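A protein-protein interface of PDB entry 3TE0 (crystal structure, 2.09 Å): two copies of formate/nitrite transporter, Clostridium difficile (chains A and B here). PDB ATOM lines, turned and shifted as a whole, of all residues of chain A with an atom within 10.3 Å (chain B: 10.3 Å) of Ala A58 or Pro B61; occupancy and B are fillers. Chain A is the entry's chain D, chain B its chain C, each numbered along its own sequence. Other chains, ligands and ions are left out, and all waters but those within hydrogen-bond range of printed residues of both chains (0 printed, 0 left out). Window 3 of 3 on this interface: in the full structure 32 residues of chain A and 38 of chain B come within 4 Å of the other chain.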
ATOM      1  N   THR A  50      -4.871 -20.937  31.915  1.00  0.00           N
ATOM      2  CA  THR A  50      -5.995 -20.666  31.025  1.00  0.00           C
ATOM      3  C   THR A  50      -5.432 -20.414  29.631  1.00  0.00           C
ATOM      4  O   THR A  50      -5.942 -20.933  28.635  1.00  0.00           O
ATOM      5  CB  THR A  50      -6.853 -19.459  31.502  1.00  0.00           C
ATOM      6  OG1 THR A  50      -7.479 -19.800  32.746  1.00  0.00           O
ATOM      7  CG2 THR A  50      -7.944 -19.136  30.472  1.00  0.00           C
ATOM      8  N   ILE A  51      -4.356 -19.632  29.581  1.00  0.00           N
ATOM      9  CA  ILE A  51      -3.638 -19.376  28.338  1.00  0.00           C
ATOM     10  C   ILE A  51      -3.059 -20.688  27.791  1.00  0.00           C
ATOM     11  O   ILE A  51      -3.165 -20.961  26.593  1.00  0.00           O
ATOM     12  CB  ILE A  51      -2.513 -18.321  28.544  1.00  0.00           C
ATOM     13  CG1 ILE A  51      -3.123 -16.934  28.782  1.00  0.00           C
ATOM     14  CG2 ILE A  51      -1.541 -18.267  27.356  1.00  0.00           C
ATOM     15  CD1 ILE A  51      -2.114 -15.911  29.312  1.00  0.00           C
ATOM     16  N   GLY A  52      -2.455 -21.494  28.663  1.00  0.00           N
ATOM     17  CA  GLY A  52      -1.906 -22.788  28.248  1.00  0.00           C
ATOM     18  C   GLY A  52      -2.958 -23.641  27.557  1.00  0.00           C
ATOM     19  O   GLY A  52      -2.729 -24.223  26.482  1.00  0.00           O
ATOM     20  N   GLY A  53      -4.140 -23.697  28.165  1.00  0.00           N
ATOM     21  CA  GLY A  53      -5.241 -24.469  27.615  1.00  0.00           C
ATOM     22  C   GLY A  53      -5.728 -23.974  26.263  1.00  0.00           C
ATOM     23  O   GLY A  53      -5.911 -24.772  25.326  1.00  0.00           O
ATOM     24  N   LEU A  54      -5.948 -22.665  26.154  1.00  0.00           N
ATOM     25  CA  LEU A  54      -6.428 -22.051  24.903  1.00  0.00           C
ATOM     26  C   LEU A  54      -5.434 -22.251  23.750  1.00  0.00           C
ATOM     27  O   LEU A  54      -5.803 -22.635  22.648  1.00  0.00           O
ATOM     28  CB  LEU A  54      -6.690 -20.547  25.112  1.00  0.00           C
ATOM     29  CG  LEU A  54      -7.874 -20.150  26.007  1.00  0.00           C
ATOM     30  CD1 LEU A  54      -7.816 -18.672  26.412  1.00  0.00           C
ATOM     31  CD2 LEU A  54      -9.201 -20.486  25.323  1.00  0.00           C
ATOM     32  N   LEU A  55      -4.162 -22.000  24.021  1.00  0.00           N
ATOM     33  CA  LEU A  55      -3.129 -22.096  22.990  1.00  0.00           C
ATOM     34  C   LEU A  55      -2.728 -23.548  22.683  1.00  0.00           C
ATOM     35  O   LEU A  55      -2.449 -23.892  21.536  1.00  0.00           O
ATOM     36  CB  LEU A  55      -1.911 -21.277  23.403  1.00  0.00           C
ATOM     37  CG  LEU A  55      -2.231 -19.788  23.565  1.00  0.00           C
ATOM     38  CD1 LEU A  55      -0.965 -19.004  23.824  1.00  0.00           C
ATOM     39  CD2 LEU A  55      -2.927 -19.270  22.321  1.00  0.00           C
ATOM     40  N   THR A  56      -2.689 -24.396  23.708  1.00  0.00           N
ATOM     41  CA  THR A  56      -2.377 -25.813  23.495  1.00  0.00           C
ATOM     42  C   THR A  56      -3.446 -26.428  22.597  1.00  0.00           C
ATOM     43  O   THR A  56      -3.139 -27.124  21.625  1.00  0.00           O
ATOM     44  CB  THR A  56      -2.284 -26.581  24.833  1.00  0.00           C
ATOM     45  OG1 THR A  56      -1.194 -26.053  25.611  1.00  0.00           O
ATOM     46  CG2 THR A  56      -2.074 -28.087  24.598  1.00  0.00           C
ATOM     47  N   ASP A  57      -4.703 -26.143  22.916  1.00  0.00           N
ATOM     48  CA  ASP A  57      -5.829 -26.595  22.097  1.00  0.00           C
ATOM     49  C   ASP A  57      -5.655 -26.145  20.644  1.00  0.00           C
ATOM     50  O   ASP A  57      -5.979 -26.881  19.708  1.00  0.00           O
ATOM     51  CB  ASP A  57      -7.148 -26.061  22.679  1.00  0.00           C
ATOM     52  CG  ASP A  57      -8.378 -26.786  22.139  1.00  0.00           C
ATOM     53  OD1 ASP A  57      -8.386 -28.038  22.097  1.00  0.00           O
ATOM     54  OD2 ASP A  57      -9.349 -26.095  21.769  1.00  0.00           O
ATOM     55  N   ALA A  58      -5.129 -24.938  20.457  1.00  0.00           N
ATOM     56  CA  ALA A  58      -4.948 -24.377  19.120  1.00  0.00           C
ATOM     57  C   ALA A  58      -3.712 -24.908  18.390  1.00  0.00           C
ATOM     58  O   ALA A  58      -3.540 -24.654  17.204  1.00  0.00           O
ATOM     59  CB  ALA A  58      -4.898 -22.850  19.194  1.00  0.00           C
ATOM     60  N   GLY A  59      -2.848 -25.628  19.099  1.00  0.00           N
ATOM     61  CA  GLY A  59      -1.604 -26.114  18.522  1.00  0.00           C
ATOM     62  C   GLY A  59      -0.564 -25.028  18.271  1.00  0.00           C
ATOM     63  O   GLY A  59       0.294 -25.176  17.403  1.00  0.00           O
ATOM     64  N   SER A  60      -0.630 -23.942  19.037  1.00  0.00           N
ATOM     65  CA  SER A  60       0.290 -22.815  18.865  1.00  0.00           C
ATOM     66  C   SER A  60       1.719 -23.154  19.310  1.00  0.00           C
ATOM     67  O   SER A  60       1.921 -23.831  20.324  1.00  0.00           O
ATOM     68  CB  SER A  60      -0.214 -21.598  19.663  1.00  0.00           C
ATOM     69  OG  SER A  60       0.754 -20.552  19.693  1.00  0.00           O
ATOM     70  N   PRO A  61       2.720 -22.675  18.558  1.00  0.00           N
ATOM     71  CA  PRO A  61       4.118 -22.829  18.986  1.00  0.00           C
ATOM     72  C   PRO A  61       4.546 -21.748  19.986  1.00  0.00           C
ATOM     73  O   PRO A  61       5.622 -21.845  20.572  1.00  0.00           O
ATOM     74  CB  PRO A  61       4.900 -22.695  17.673  1.00  0.00           C
ATOM     75  CG  PRO A  61       4.046 -21.817  16.825  1.00  0.00           C
ATOM     76  CD  PRO A  61       2.607 -22.099  17.206  1.00  0.00           C
ATOM     77  N   MET A  62       3.695 -20.746  20.186  1.00  0.00           N
ATOM     78  CA  MET A  62       3.979 -19.629  21.084  1.00  0.00           C
ATOM     79  C   MET A  62       3.453 -19.834  22.516  1.00  0.00           C
ATOM     80  O   MET A  62       3.619 -18.968  23.369  1.00  0.00           O
ATOM     81  CB  MET A  62       3.393 -18.335  20.504  1.00  0.00           C
ATOM     82  CG  MET A  62       4.077 -17.839  19.227  1.00  0.00           C
ATOM     83  SD  MET A  62       5.650 -16.980  19.523  1.00  0.00           S
ATOM     84  CE  MET A  62       5.133 -15.515  20.418  1.00  0.00           C
ATOM     85  N   THR A  63       2.830 -20.978  22.771  1.00  0.00           N
ATOM     86  CA  THR A  63       2.180 -21.255  24.052  1.00  0.00           C
ATOM     87  C   THR A  63       3.040 -20.895  25.274  1.00  0.00           C
ATOM     88  O   THR A  63       2.631 -20.104  26.118  1.00  0.00           O
ATOM     89  CB  THR A  63       1.770 -22.750  24.176  1.00  0.00           C
ATOM     90  OG1 THR A  63       0.868 -23.097  23.121  1.00  0.00           O
ATOM     91  CG2 THR A  63       1.086 -23.015  25.532  1.00  0.00           C
ATOM     92  N   VAL A  66       3.981 -17.072  25.514  1.00  0.00           N
ATOM     93  CA  VAL A  66       2.886 -16.233  25.986  1.00  0.00           C
ATOM     94  C   VAL A  66       2.597 -16.506  27.475  1.00  0.00           C
ATOM     95  O   VAL A  66       2.235 -15.598  28.230  1.00  0.00           O
ATOM     96  CB  VAL A  66       1.622 -16.442  25.126  1.00  0.00           C
ATOM     97  CG1 VAL A  66       0.467 -15.579  25.649  1.00  0.00           C
ATOM     98  CG2 VAL A  66       1.936 -16.096  23.654  1.00  0.00           C
ATOM     99  N   PRO A 139     -10.454 -27.464  27.375  1.00  0.00           N
ATOM    100  CA  PRO A 139      -8.995 -27.340  27.263  1.00  0.00           C
ATOM    101  C   PRO A 139      -8.301 -26.848  28.541  1.00  0.00           C
ATOM    102  O   PRO A 139      -7.192 -27.298  28.824  1.00  0.00           O
ATOM    103  CB  PRO A 139      -8.802 -26.349  26.102  1.00  0.00           C
ATOM    104  CG  PRO A 139     -10.184 -25.844  25.749  1.00  0.00           C
ATOM    105  CD  PRO A 139     -11.159 -26.864  26.229  1.00  0.00           C
ATOM    106  N   VAL A 140      -8.932 -25.964  29.309  1.00  0.00           N
ATOM    107  CA  VAL A 140      -8.270 -25.457  30.508  1.00  0.00           C
ATOM    108  C   VAL A 140      -8.207 -26.543  31.566  1.00  0.00           C
ATOM    109  O   VAL A 140      -7.151 -26.781  32.169  1.00  0.00           O
ATOM    110  CB  VAL A 140      -8.930 -24.173  31.045  1.00  0.00           C
ATOM    111  CG1 VAL A 140      -8.181 -23.661  32.268  1.00  0.00           C
ATOM    112  CG2 VAL A 140      -8.976 -23.115  29.940  1.00  0.00           C
ATOM    113  N   GLU A 142      -8.225 -29.677  31.023  1.00  0.00           N
ATOM    114  CA  GLU A 142      -7.258 -30.682  30.562  1.00  0.00           C
ATOM    115  C   GLU A 142      -5.805 -30.214  30.747  1.00  0.00           C
ATOM    116  O   GLU A 142      -4.925 -31.009  31.078  1.00  0.00           O
ATOM    117  CB  GLU A 142      -7.557 -31.098  29.112  1.00  0.00           C
ATOM    118  CG  GLU A 142      -8.946 -31.752  28.998  1.00  0.00           C
ATOM    119  CD  GLU A 142      -9.319 -32.196  27.590  1.00  0.00           C
ATOM    120  OE1 GLU A 142      -8.418 -32.346  26.738  1.00  0.00           O
ATOM    121  OE2 GLU A 142     -10.529 -32.400  27.338  1.00  0.00           O
ATOM    122  N   PHE A 143      -5.561 -28.923  30.564  1.00  0.00           N
ATOM    123  CA  PHE A 143      -4.215 -28.388  30.779  1.00  0.00           C
ATOM    124  C   PHE A 143      -3.768 -28.566  32.231  1.00  0.00           C
ATOM    125  O   PHE A 143      -2.644 -29.007  32.479  1.00  0.00           O
ATOM    126  CB  PHE A 143      -4.105 -26.925  30.338  1.00  0.00           C
ATOM    127  CG  PHE A 143      -2.679 -26.452  30.180  1.00  0.00           C
ATOM    128  CD1 PHE A 143      -1.978 -26.690  29.000  1.00  0.00           C
ATOM    129  CD2 PHE A 143      -2.028 -25.801  31.223  1.00  0.00           C
ATOM    130  CE1 PHE A 143      -0.663 -26.270  28.853  1.00  0.00           C
ATOM    131  CE2 PHE A 143      -0.707 -25.388  31.089  1.00  0.00           C
ATOM    132  CZ  PHE A 143      -0.024 -25.611  29.896  1.00  0.00           C
ATOM    133  N   ILE B  51     -13.450  -6.088  20.014  1.00  0.00           N
ATOM    134  CA  ILE B  51     -12.371  -7.023  19.781  1.00  0.00           C
ATOM    135  C   ILE B  51     -12.887  -8.471  19.754  1.00  0.00           C
ATOM    136  O   ILE B  51     -12.544  -9.231  18.857  1.00  0.00           O
ATOM    137  CB  ILE B  51     -11.256  -6.853  20.842  1.00  0.00           C
ATOM    138  CG1 ILE B  51     -10.521  -5.528  20.588  1.00  0.00           C
ATOM    139  CG2 ILE B  51     -10.272  -8.046  20.773  1.00  0.00           C
ATOM    140  CD1 ILE B  51      -9.553  -5.103  21.687  1.00  0.00           C
ATOM    141  N   GLY B  52     -13.715  -8.833  20.730  1.00  0.00           N
ATOM    142  CA  GLY B  52     -14.366 -10.130  20.746  1.00  0.00           C
ATOM    143  C   GLY B  52     -15.058 -10.442  19.426  1.00  0.00           C
ATOM    144  O   GLY B  52     -14.846 -11.507  18.844  1.00  0.00           O
ATOM    145  N   LEU B  54     -14.692  -8.974  16.392  1.00  0.00           N
ATOM    146  CA  LEU B  54     -13.682  -9.052  15.341  1.00  0.00           C
ATOM    147  C   LEU B  54     -12.944 -10.397  15.310  1.00  0.00           C
ATOM    148  O   LEU B  54     -12.815 -11.018  14.258  1.00  0.00           O
ATOM    149  CB  LEU B  54     -12.679  -7.904  15.491  1.00  0.00           C
ATOM    150  CG  LEU B  54     -13.188  -6.504  15.147  1.00  0.00           C
ATOM    151  CD1 LEU B  54     -12.181  -5.421  15.560  1.00  0.00           C
ATOM    152  CD2 LEU B  54     -13.492  -6.429  13.653  1.00  0.00           C
ATOM    153  N   LEU B  55     -12.472 -10.865  16.461  1.00  0.00           N
ATOM    154  CA  LEU B  55     -11.634 -12.067  16.482  1.00  0.00           C
ATOM    155  C   LEU B  55     -12.420 -13.382  16.523  1.00  0.00           C
ATOM    156  O   LEU B  55     -11.928 -14.433  16.104  1.00  0.00           O
ATOM    157  CB  LEU B  55     -10.646 -11.995  17.642  1.00  0.00           C
ATOM    158  CG  LEU B  55      -9.688 -10.802  17.573  1.00  0.00           C
ATOM    159  CD1 LEU B  55      -8.663 -10.842  18.716  1.00  0.00           C
ATOM    160  CD2 LEU B  55      -8.996 -10.732  16.213  1.00  0.00           C
ATOM    161  N   THR B  56     -13.633 -13.334  17.060  1.00  0.00           N
ATOM    162  CA  THR B  56     -14.471 -14.522  17.088  1.00  0.00           C
ATOM    163  C   THR B  56     -14.896 -14.837  15.660  1.00  0.00           C
ATOM    164  O   THR B  56     -14.762 -15.974  15.192  1.00  0.00           O
ATOM    165  CB  THR B  56     -15.691 -14.337  18.004  1.00  0.00           C
ATOM    166  OG1 THR B  56     -15.242 -14.148  19.357  1.00  0.00           O
ATOM    167  CG2 THR B  56     -16.617 -15.558  17.931  1.00  0.00           C
ATOM    168  N   ASP B  57     -15.374 -13.817  14.958  1.00  0.00           N
ATOM    169  CA  ASP B  57     -15.757 -13.970  13.563  1.00  0.00           C
ATOM    170  C   ASP B  57     -14.620 -14.625  12.770  1.00  0.00           C
ATOM    171  O   ASP B  57     -14.854 -15.382  11.812  1.00  0.00           O
ATOM    172  CB  ASP B  57     -16.092 -12.602  12.966  1.00  0.00           C
ATOM    173  CG  ASP B  57     -16.898 -12.704  11.681  1.00  0.00           C
ATOM    174  OD1 ASP B  57     -17.913 -13.435  11.671  1.00  0.00           O
ATOM    175  OD2 ASP B  57     -16.514 -12.046  10.688  1.00  0.00           O
ATOM    176  N   ALA B  58     -13.390 -14.341  13.187  1.00  0.00           N
ATOM    177  CA  ALA B  58     -12.205 -14.769  12.443  1.00  0.00           C
ATOM    178  C   ALA B  58     -11.648 -16.125  12.885  1.00  0.00           C
ATOM    179  O   ALA B  58     -10.752 -16.670  12.243  1.00  0.00           O
ATOM    180  CB  ALA B  58     -11.119 -13.686  12.512  1.00  0.00           C
ATOM    181  N   GLY B  59     -12.164 -16.651  13.992  1.00  0.00           N
ATOM    182  CA  GLY B  59     -11.747 -17.946  14.510  1.00  0.00           C
ATOM    183  C   GLY B  59     -10.473 -17.958  15.348  1.00  0.00           C
ATOM    184  O   GLY B  59      -9.925 -19.022  15.650  1.00  0.00           O
ATOM    185  N   SER B  60      -9.998 -16.780  15.729  1.00  0.00           N
ATOM    186  CA  SER B  60      -8.731 -16.667  16.438  1.00  0.00           C
ATOM    187  C   SER B  60      -8.724 -17.406  17.791  1.00  0.00           C
ATOM    188  O   SER B  60      -9.694 -17.343  18.543  1.00  0.00           O
ATOM    189  CB  SER B  60      -8.392 -15.184  16.652  1.00  0.00           C
ATOM    190  OG  SER B  60      -7.147 -15.053  17.315  1.00  0.00           O
ATOM    191  N   PRO B  61      -7.620 -18.104  18.107  1.00  0.00           N
ATOM    192  CA  PRO B  61      -7.489 -18.689  19.446  1.00  0.00           C
ATOM    193  C   PRO B  61      -6.961 -17.666  20.473  1.00  0.00           C
ATOM    194  O   PRO B  61      -6.918 -17.965  21.665  1.00  0.00           O
ATOM    195  CB  PRO B  61      -6.459 -19.797  19.227  1.00  0.00           C
ATOM    196  CG  PRO B  61      -5.559 -19.234  18.176  1.00  0.00           C
ATOM    197  CD  PRO B  61      -6.449 -18.403  17.261  1.00  0.00           C
ATOM    198  N   MET B  62      -6.569 -16.483  20.007  1.00  0.00           N
ATOM    199  CA  MET B  62      -6.013 -15.436  20.874  1.00  0.00           C
ATOM    200  C   MET B  62      -7.091 -14.474  21.397  1.00  0.00           C
ATOM    201  O   MET B  62      -6.812 -13.556  22.178  1.00  0.00           O
ATOM    202  CB  MET B  62      -4.927 -14.650  20.123  1.00  0.00           C
ATOM    203  CG  MET B  62      -3.645 -15.447  19.848  1.00  0.00           C
ATOM    204  SD  MET B  62      -2.537 -15.562  21.281  1.00  0.00           S
ATOM    205  CE  MET B  62      -2.323 -13.836  21.718  1.00  0.00           C
ATOM    206  N   THR B  63      -8.325 -14.697  20.962  1.00  0.00           N
ATOM    207  CA  THR B  63      -9.436 -13.816  21.293  1.00  0.00           C
ATOM    208  C   THR B  63      -9.506 -13.375  22.766  1.00  0.00           C
ATOM    209  O   THR B  63      -9.443 -12.175  23.073  1.00  0.00           O
ATOM    210  CB  THR B  63     -10.763 -14.456  20.880  1.00  0.00           C
ATOM    211  OG1 THR B  63     -10.717 -14.731  19.475  1.00  0.00           O
ATOM    212  CG2 THR B  63     -11.941 -13.520  21.208  1.00  0.00           C
ATOM    213  N   LYS B  64      -9.657 -14.336  23.671  1.00  0.00           N
ATOM    214  CA  LYS B  64      -9.809 -14.020  25.093  1.00  0.00           C
ATOM    215  C   LYS B  64      -8.527 -13.424  25.683  1.00  0.00           C
ATOM    216  O   LYS B  64      -8.589 -12.698  26.660  1.00  0.00           O
ATOM    217  CB  LYS B  64     -10.217 -15.256  25.901  1.00  0.00           C
ATOM    218  CG  LYS B  64     -11.594 -15.825  25.566  1.00  0.00           C
ATOM    219  CD  LYS B  64     -11.712 -17.266  26.084  1.00  0.00           C
ATOM    220  CE  LYS B  64     -13.058 -17.919  25.749  1.00  0.00           C
ATOM    221  NZ  LYS B  64     -14.186 -17.320  26.508  1.00  0.00           N
ATOM    222  N   ILE B  65      -7.370 -13.754  25.112  1.00  0.00           N
ATOM    223  CA  ILE B  65      -6.111 -13.169  25.588  1.00  0.00           C
ATOM    224  C   ILE B  65      -6.020 -11.690  25.216  1.00  0.00           C
ATOM    225  O   ILE B  65      -5.669 -10.838  26.039  1.00  0.00           O
ATOM    226  CB  ILE B  65      -4.872 -13.925  25.040  1.00  0.00           C
ATOM    227  CG1 ILE B  65      -4.872 -15.372  25.534  1.00  0.00           C
ATOM    228  CG2 ILE B  65      -3.563 -13.211  25.457  1.00  0.00           C
ATOM    229  CD1 ILE B  65      -3.990 -16.292  24.712  1.00  0.00           C
ATOM    230  N   VAL B  66      -6.332 -11.390  23.957  1.00  0.00           N
ATOM    231  CA  VAL B  66      -6.333 -10.025  23.487  1.00  0.00           C
ATOM    232  C   VAL B  66      -7.384  -9.192  24.224  1.00  0.00           C
ATOM    233  O   VAL B  66      -7.153  -8.028  24.538  1.00  0.00           O
ATOM    234  CB  VAL B  66      -6.530  -9.943  21.955  1.00  0.00           C
ATOM    235  CG1 VAL B  66      -6.556  -8.478  21.499  1.00  0.00           C
ATOM    236  CG2 VAL B  66      -5.404 -10.736  21.224  1.00  0.00           C
ATOM    237  N   MET B  67      -8.531  -9.785  24.518  1.00  0.00           N
ATOM    238  CA  MET B  67      -9.553  -9.043  25.255  1.00  0.00           C
ATOM    239  C   MET B  67      -9.033  -8.671  26.644  1.00  0.00           C
ATOM    240  O   MET B  67      -9.221  -7.543  27.103  1.00  0.00           O
ATOM    241  CB  MET B  67     -10.843  -9.864  25.379  1.00  0.00           C
ATOM    242  CG  MET B  67     -11.639  -9.974  24.067  1.00  0.00           C
ATOM    243  SD  MET B  67     -13.052 -11.094  24.222  1.00  0.00           S
ATOM    244  CE  MET B  67     -14.058 -10.255  25.460  1.00  0.00           C
ATOM    245  N   GLY B  68      -8.397  -9.627  27.322  1.00  0.00           N
ATOM    246  CA  GLY B  68      -7.863  -9.362  28.657  1.00  0.00           C
ATOM    247  C   GLY B  68      -6.807  -8.266  28.640  1.00  0.00           C
ATOM    248  O   GLY B  68      -6.796  -7.371  29.487  1.00  0.00           O
ATOM    249  N   THR B 199      -9.203 -12.568  31.151  1.00  0.00           N
ATOM    250  CA  THR B 199      -8.788 -13.744  30.391  1.00  0.00           C
ATOM    251  C   THR B 199      -9.117 -15.040  31.135  1.00  0.00           C
ATOM    252  O   THR B 199      -9.456 -16.057  30.518  1.00  0.00           O
ATOM    253  CB  THR B 199      -7.290 -13.656  30.017  1.00  0.00           C
ATOM    254  OG1 THR B 199      -7.117 -12.529  29.148  1.00  0.00           O
ATOM    255  CG2 THR B 199      -6.808 -14.942  29.300  1.00  0.00           C
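Of the printed residues of chain B, Thr A50 touches Thr B199. Ile A51 touches none of the printed residues of chain B. Gly A53 touches none of the printed residues of chain B. Of the printed residues of chain B, Leu A55 touches Met B62 (3.9 Å) and Ile B65 (3.96 Å). No residue of chain B comes within 4 Å of Asp A57. Ala A58 touches just one residue of chain B: Pro B61. No residue of chain B comes within 4 Å of Gly A59. No residue of chain B comes within 4 Å of Ser A60. Of the printed residues of chain A, Pro B61 touches Ala A58. Of the printed residues of chain A, Ile B65 touches Leu A55. Of the printed residues of chain A, Thr B199 touches Thr A50 (3.4 Å). The nearest residue of chain A that does not touch Pro B61 is Leu A55 (4.2 Å). The nearest printed residue of chain A that does not touch Ile B65 is Ile A51 (4.01 Å).
The backbone NH (N) of Met B62 lies within hydrogen-bond range of the side-chain hydroxyl (OG) of Ser B60, at 3.1 Å. O of Leu A55 sits at hydrogen-bond distance from N of Ser A60 (3.1 Å). The backbone carbonyl oxygen (O) of Lys B64 sits at hydrogen-bond distance from the side-chain hydroxyl (OG1) of Thr B199.
CG2 of Thr A50 touches O of Thr B199 (3.4 Å). CD2 of Leu A55 touches SD of Met B62 (3.9 Å). Leu A55 touches Ile B65. Pro B61 touches Ala A58.
Leu A55 touches Met B62, but with the chains exchanged Met A62 does not touch Leu B55 (14.3 Å). Ala A58 touches Pro B61, but with the chains exchanged Pro A61 does not touch Ala B58 (15.3 Å). Positions printed for both chains: 51, 52, 54, 55, 56, 57, 58, 59, 60, 61, 62, 63 and 66. Of the 4 pairs that touch across the chains among the printed residues, none has its exchanged pair printed and touching as well.
Of the 18 printed residues of chain B, 4 touch a printed residue of chain A. Of the 19 printed residues of chain A, 3 touch a printed residue of chain B. Hydrophobic or aromatic side chains of chain A within 4 Å of the printed part of chain B: Leu A55 and Ala A58. Among the printed residues, 4 pairs touch across the chains. Among the printed residues, no Asp or Glu carboxylate lies within 4 Å of a Lys or Arg side-chain nitrogen of the other chain.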
